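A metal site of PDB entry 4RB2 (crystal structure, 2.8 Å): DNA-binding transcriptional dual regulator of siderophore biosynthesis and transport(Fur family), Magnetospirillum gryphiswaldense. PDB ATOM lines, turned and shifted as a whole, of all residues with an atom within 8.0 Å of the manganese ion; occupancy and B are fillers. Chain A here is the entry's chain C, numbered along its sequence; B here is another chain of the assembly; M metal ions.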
ATOM      1  N   HIS A  89     -10.124   8.771 -10.316  1.00  0.00           N
ATOM      2  CA  HIS A  89      -9.108   8.519  -9.294  1.00  0.00           C
ATOM      3  C   HIS A  89      -8.259   7.322  -9.678  1.00  0.00           C
ATOM      4  O   HIS A  89      -8.751   6.345 -10.244  1.00  0.00           O
ATOM      5  CB  HIS A  89      -9.730   8.265  -7.921  1.00  0.00           C
ATOM      6  CG  HIS A  89      -8.819   7.553  -6.969  1.00  0.00           C
ATOM      7  ND1 HIS A  89      -7.784   8.180  -6.308  1.00  0.00           N
ATOM      8  CD2 HIS A  89      -8.775   6.249  -6.589  1.00  0.00           C
ATOM      9  CE1 HIS A  89      -7.152   7.301  -5.559  1.00  0.00           C
ATOM     10  NE2 HIS A  89      -7.731   6.121  -5.706  1.00  0.00           N
ATOM     11  N   HIS A  90      -6.973   7.403  -9.360  1.00  0.00           N
ATOM     12  CA  HIS A  90      -6.046   6.303  -9.579  1.00  0.00           C
ATOM     13  C   HIS A  90      -4.919   6.398  -8.563  1.00  0.00           C
ATOM     14  O   HIS A  90      -4.687   7.458  -7.959  1.00  0.00           O
ATOM     15  CB  HIS A  90      -5.493   6.352 -11.011  1.00  0.00           C
ATOM     16  CG  HIS A  90      -4.743   7.609 -11.315  1.00  0.00           C
ATOM     17  ND1 HIS A  90      -5.368   8.801 -11.584  1.00  0.00           N
ATOM     18  CD2 HIS A  90      -3.418   7.852 -11.401  1.00  0.00           C
ATOM     19  CE1 HIS A  90      -4.459   9.733 -11.822  1.00  0.00           C
ATOM     20  NE2 HIS A  90      -3.258   9.182 -11.709  1.00  0.00           N
ATOM     21  N   ASP A  91      -4.224   5.285  -8.377  1.00  0.00           N
ATOM     22  CA  ASP A  91      -3.028   5.280  -7.540  1.00  0.00           C
ATOM     23  C   ASP A  91      -1.800   5.253  -8.450  1.00  0.00           C
ATOM     24  O   ASP A  91      -1.924   5.504  -9.655  1.00  0.00           O
ATOM     25  CB  ASP A  91      -3.077   4.084  -6.587  1.00  0.00           C
ATOM     26  CG  ASP A  91      -4.470   3.879  -5.987  1.00  0.00           C
ATOM     27  OD1 ASP A  91      -5.068   4.875  -5.528  1.00  0.00           O
ATOM     28  OD2 ASP A  91      -4.963   2.738  -5.987  1.00  0.00           O
ATOM     29  N   HIS A  92      -0.612   4.972  -7.910  1.00  0.00           N
ATOM     30  CA  HIS A  92       0.594   4.985  -8.737  1.00  0.00           C
ATOM     31  C   HIS A  92       1.553   3.811  -8.492  1.00  0.00           C
ATOM     32  O   HIS A  92       1.788   3.388  -7.357  1.00  0.00           O
ATOM     33  CB  HIS A  92       1.355   6.311  -8.623  1.00  0.00           C
ATOM     34  CG  HIS A  92       0.503   7.504  -8.871  1.00  0.00           C
ATOM     35  ND1 HIS A  92      -0.242   8.098  -7.874  1.00  0.00           N
ATOM     36  CD2 HIS A  92       0.248   8.201  -9.999  1.00  0.00           C
ATOM     37  CE1 HIS A  92      -0.915   9.128  -8.379  1.00  0.00           C
ATOM     38  NE2 HIS A  92      -0.633   9.208  -9.669  1.00  0.00           N
ATOM     39  N   PHE A 104      -2.860   3.262 -12.150  1.00  0.00           N
ATOM     40  CA  PHE A 104      -3.770   2.114 -11.997  1.00  0.00           C
ATOM     41  C   PHE A 104      -4.934   2.314 -11.025  1.00  0.00           C
ATOM     42  O   PHE A 104      -4.903   3.157 -10.119  1.00  0.00           O
ATOM     43  CB  PHE A 104      -2.982   0.851 -11.602  1.00  0.00           C
ATOM     44  CG  PHE A 104      -2.645   0.775 -10.130  1.00  0.00           C
ATOM     45  CD1 PHE A 104      -1.517   1.421  -9.632  1.00  0.00           C
ATOM     46  CD2 PHE A 104      -3.451   0.054  -9.250  1.00  0.00           C
ATOM     47  CE1 PHE A 104      -1.203   1.354  -8.282  1.00  0.00           C
ATOM     48  CE2 PHE A 104      -3.143  -0.010  -7.908  1.00  0.00           C
ATOM     49  CZ  PHE A 104      -2.020   0.638  -7.417  1.00  0.00           C
ATOM     50  N   THR A 105      -5.963   1.494 -11.238  1.00  0.00           N
ATOM     51  CA  THR A 105      -7.142   1.450 -10.391  1.00  0.00           C
ATOM     52  C   THR A 105      -7.399   0.004 -10.009  1.00  0.00           C
ATOM     53  O   THR A 105      -7.377  -0.879 -10.878  1.00  0.00           O
ATOM     54  CB  THR A 105      -8.392   1.991 -11.132  1.00  0.00           C
ATOM     55  OG1 THR A 105      -8.443   1.449 -12.458  1.00  0.00           O
ATOM     56  CG2 THR A 105      -8.389   3.509 -11.202  1.00  0.00           C
ATOM     57  N   SER A 106      -7.614  -0.250  -8.732  1.00  0.00           N
ATOM     58  CA  SER A 106      -8.039  -1.566  -8.294  1.00  0.00           C
ATOM     59  C   SER A 106      -9.230  -1.366  -7.381  1.00  0.00           C
ATOM     60  O   SER A 106      -9.067  -0.973  -6.231  1.00  0.00           O
ATOM     61  CB  SER A 106      -6.929  -2.306  -7.572  1.00  0.00           C
ATOM     62  OG  SER A 106      -7.387  -3.544  -7.067  1.00  0.00           O
ATOM     63  N   PRO A 107     -10.444  -1.645  -7.905  1.00  0.00           N
ATOM     64  CA  PRO A 107     -11.686  -1.430  -7.155  1.00  0.00           C
ATOM     65  C   PRO A 107     -11.741  -2.272  -5.877  1.00  0.00           C
ATOM     66  O   PRO A 107     -12.339  -1.843  -4.882  1.00  0.00           O
ATOM     67  CB  PRO A 107     -12.776  -1.875  -8.143  1.00  0.00           C
ATOM     68  CG  PRO A 107     -12.113  -1.866  -9.488  1.00  0.00           C
ATOM     69  CD  PRO A 107     -10.699  -2.260  -9.219  1.00  0.00           C
ATOM     70  N   ILE A 109      -9.154  -3.058  -3.890  1.00  0.00           N
ATOM     71  CA  ILE A 109      -8.342  -2.361  -2.887  1.00  0.00           C
ATOM     72  C   ILE A 109      -9.120  -1.185  -2.293  1.00  0.00           C
ATOM     73  O   ILE A 109      -9.258  -1.083  -1.071  1.00  0.00           O
ATOM     74  CB  ILE A 109      -7.003  -1.859  -3.473  1.00  0.00           C
ATOM     75  CG1 ILE A 109      -6.157  -3.038  -3.949  1.00  0.00           C
ATOM     76  CG2 ILE A 109      -6.242  -1.034  -2.422  1.00  0.00           C
ATOM     77  CD1 ILE A 109      -4.776  -2.667  -4.436  1.00  0.00           C
ATOM     78  N   GLU A 110      -9.635  -0.342  -3.178  1.00  0.00           N
ATOM     79  CA  GLU A 110     -10.480   0.793  -2.797  1.00  0.00           C
ATOM     80  C   GLU A 110     -11.624   0.318  -1.901  1.00  0.00           C
ATOM     81  O   GLU A 110     -12.059   1.047  -1.019  1.00  0.00           O
ATOM     82  CB  GLU A 110     -11.052   1.489  -4.036  1.00  0.00           C
ATOM     83  CG  GLU A 110     -10.078   1.648  -5.206  1.00  0.00           C
ATOM     84  CD  GLU A 110      -9.009   2.705  -4.993  1.00  0.00           C
ATOM     85  OE1 GLU A 110      -7.970   2.624  -5.686  1.00  0.00           O
ATOM     86  OE2 GLU A 110      -9.201   3.619  -4.158  1.00  0.00           O
ATOM     87  N   ALA A 111     -12.086  -0.908  -2.150  1.00  0.00           N
ATOM     88  CA  ALA A 111     -13.185  -1.495  -1.382  1.00  0.00           C
ATOM     89  C   ALA A 111     -12.705  -2.108  -0.071  1.00  0.00           C
ATOM     90  O   ALA A 111     -13.410  -2.038   0.935  1.00  0.00           O
ATOM     91  CB  ALA A 111     -13.928  -2.526  -2.218  1.00  0.00           C
ATOM     92  N   GLN A 113     -10.163  -0.978   1.433  1.00  0.00           N
ATOM     93  CA  GLN A 113      -9.853   0.241   2.174  1.00  0.00           C
ATOM     94  C   GLN A 113     -11.088   0.690   2.947  1.00  0.00           C
ATOM     95  O   GLN A 113     -11.004   0.937   4.159  1.00  0.00           O
ATOM     96  CB  GLN A 113      -9.384   1.358   1.239  1.00  0.00           C
ATOM     97  CG  GLN A 113      -7.978   1.169   0.680  1.00  0.00           C
ATOM     98  CD  GLN A 113      -7.659   2.131  -0.442  1.00  0.00           C
ATOM     99  OE1 GLN A 113      -6.645   1.982  -1.145  1.00  0.00           O
ATOM    100  NE2 GLN A 113      -8.516   3.123  -0.650  1.00  0.00           N
ATOM    101  N   GLY A 126     -10.234   9.906   2.530  1.00  0.00           N
ATOM    102  CA  GLY A 126      -9.105  10.013   1.601  1.00  0.00           C
ATOM    103  C   GLY A 126      -8.072   8.911   1.823  1.00  0.00           C
ATOM    104  O   GLY A 126      -8.083   8.241   2.866  1.00  0.00           O
ATOM    105  N   HIS A 127      -7.195   8.728   0.842  1.00  0.00           N
ATOM    106  CA  HIS A 127      -6.156   7.701   0.921  1.00  0.00           C
ATOM    107  C   HIS A 127      -5.013   7.984  -0.037  1.00  0.00           C
ATOM    108  O   HIS A 127      -5.201   8.603  -1.077  1.00  0.00           O
ATOM    109  CB  HIS A 127      -6.740   6.303   0.665  1.00  0.00           C
ATOM    110  CG  HIS A 127      -7.026   6.025  -0.777  1.00  0.00           C
ATOM    111  ND1 HIS A 127      -8.133   6.518  -1.419  1.00  0.00           N
ATOM    112  CD2 HIS A 127      -6.338   5.298  -1.696  1.00  0.00           C
ATOM    113  CE1 HIS A 127      -8.127   6.117  -2.679  1.00  0.00           C
ATOM    114  NE2 HIS A 127      -7.056   5.371  -2.873  1.00  0.00           N
ATOM    115  N   ARG A 128      -3.825   7.503   0.332  1.00  0.00           N
ATOM    116  CA  ARG A 128      -2.661   7.524  -0.538  1.00  0.00           C
ATOM    117  C   ARG A 128      -2.201   6.097  -0.775  1.00  0.00           C
ATOM    118  O   ARG A 128      -2.124   5.290   0.166  1.00  0.00           O
ATOM    119  CB  ARG A 128      -1.524   8.331   0.082  1.00  0.00           C
ATOM    120  CG  ARG A 128      -0.488   8.799  -0.920  1.00  0.00           C
ATOM    121  CD  ARG A 128       0.764   9.345  -0.252  1.00  0.00           C
ATOM    122  NE  ARG A 128       0.513  10.209   0.902  1.00  0.00           N
ATOM    123  CZ  ARG A 128       1.333  11.163   1.342  1.00  0.00           C
ATOM    124  NH1 ARG A 128       2.483  11.407   0.711  1.00  0.00           N
ATOM    125  NH2 ARG A 128       0.993  11.889   2.400  1.00  0.00           N
ATOM    126  N   LEU A 129      -1.883   5.792  -2.025  1.00  0.00           N
ATOM    127  CA  LEU A 129      -1.284   4.500  -2.345  1.00  0.00           C
ATOM    128  C   LEU A 129      -0.232   4.660  -3.416  1.00  0.00           C
ATOM    129  O   LEU A 129      -0.442   5.347  -4.426  1.00  0.00           O
ATOM    130  CB  LEU A 129      -2.344   3.476  -2.772  1.00  0.00           C
ATOM    131  CG  LEU A 129      -1.883   2.044  -3.062  1.00  0.00           C
ATOM    132  CD1 LEU A 129      -1.315   1.360  -1.828  1.00  0.00           C
ATOM    133  CD2 LEU A 129      -3.055   1.256  -3.625  1.00  0.00           C
ATOM    134  N   GLU A 130       0.915   4.050  -3.159  1.00  0.00           N
ATOM    135  CA  GLU A 130       2.032   4.057  -4.066  1.00  0.00           C
ATOM    136  C   GLU A 130       2.709   2.712  -3.973  1.00  0.00           C
ATOM    137  O   GLU A 130       2.983   2.223  -2.878  1.00  0.00           O
ATOM    138  CB  GLU A 130       2.989   5.187  -3.705  1.00  0.00           C
ATOM    139  CG  GLU A 130       2.548   6.520  -4.293  1.00  0.00           C
ATOM    140  CD  GLU A 130       2.777   7.698  -3.356  1.00  0.00           C
ATOM    141  OE1 GLU A 130       1.846   8.522  -3.231  1.00  0.00           O
ATOM    142  OE2 GLU A 130       3.869   7.793  -2.767  1.00  0.00           O
ATOM    143  N   LEU B 129       0.912   2.860   1.943  1.00  0.00           N
ATOM    144  CA  LEU B 129      -0.549   3.055   2.027  1.00  0.00           C
ATOM    145  C   LEU B 129      -0.967   3.810   3.295  1.00  0.00           C
ATOM    146  O   LEU B 129      -0.823   3.299   4.409  1.00  0.00           O
ATOM    147  CB  LEU B 129      -1.325   1.737   1.927  1.00  0.00           C
ATOM    148  CG  LEU B 129      -2.828   1.692   2.294  1.00  0.00           C
ATOM    149  CD1 LEU B 129      -3.672   2.670   1.477  1.00  0.00           C
ATOM    150  CD2 LEU B 129      -3.395   0.287   2.153  1.00  0.00           C
ATOM    151  N   GLU B 130      -1.476   5.020   3.093  1.00  0.00           N
ATOM    152  CA  GLU B 130      -2.102   5.804   4.146  1.00  0.00           C
ATOM    153  C   GLU B 130      -3.587   5.834   3.924  1.00  0.00           C
ATOM    154  O   GLU B 130      -4.052   6.136   2.827  1.00  0.00           O
ATOM    155  CB  GLU B 130      -1.598   7.245   4.128  1.00  0.00           C
ATOM    156  CG  GLU B 130      -0.497   7.542   5.113  1.00  0.00           C
ATOM    157  CD  GLU B 130       0.860   7.364   4.503  1.00  0.00           C
ATOM    158  OE1 GLU B 130       1.335   6.211   4.430  1.00  0.00           O
ATOM    159  OE2 GLU B 130       1.449   8.389   4.091  1.00  0.00           O
ATOM    160  N   LEU B 131      -4.347   5.546   4.982  1.00  0.00           N
ATOM    161  CA  LEU B 131      -5.775   5.792   4.960  1.00  0.00           C
ATOM    162  C   LEU B 131      -6.060   7.019   5.805  1.00  0.00           C
ATOM    163  O   LEU B 131      -5.444   7.211   6.849  1.00  0.00           O
ATOM    164  CB  LEU B 131      -6.561   4.592   5.469  1.00  0.00           C
ATOM    165  CG  LEU B 131      -6.576   3.333   4.605  1.00  0.00           C
ATOM    166  CD1 LEU B 131      -7.585   2.334   5.133  1.00  0.00           C
ATOM    167  CD2 LEU B 131      -6.879   3.679   3.165  1.00  0.00           C
HETATM  168 MN    MN M   1      -6.622   4.349  -4.438  1.00  0.00          MN
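A ring nitrogen (NE2) of His 127 sits close to the side-chain amide nitrogen of Gln 113, at 3.5 Å.
The backbone NH of Asp 91 is in hydrogen-bond range of the backbone carbonyl oxygen of Phe 104.
Four residues have an atom within 4 Å of the manganese ion: His 89, Asp 91, Glu 110 and His 127.
The nearest printed residue that does not touch the manganese ion is Gln 113 (4.1 Å).
NE2 of His 127 binds the manganese ion, 1.9 Å away.
OD1 of Asp 91 binds the manganese ion, 2.0 Å away.
The manganese ion is bound by NE2 of His 89, 2.4 Å away.
The manganese ion is bound by OE1 of Glu 110 (2.5 Å).
The side-chain carboxylate (OE2) of Glu 110 is bound to the manganese ion, at 2.7 Å.
Slightly farther from the manganese ion lies the side-chain carboxylate (OD2) of Asp 91 (2.8 Å).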
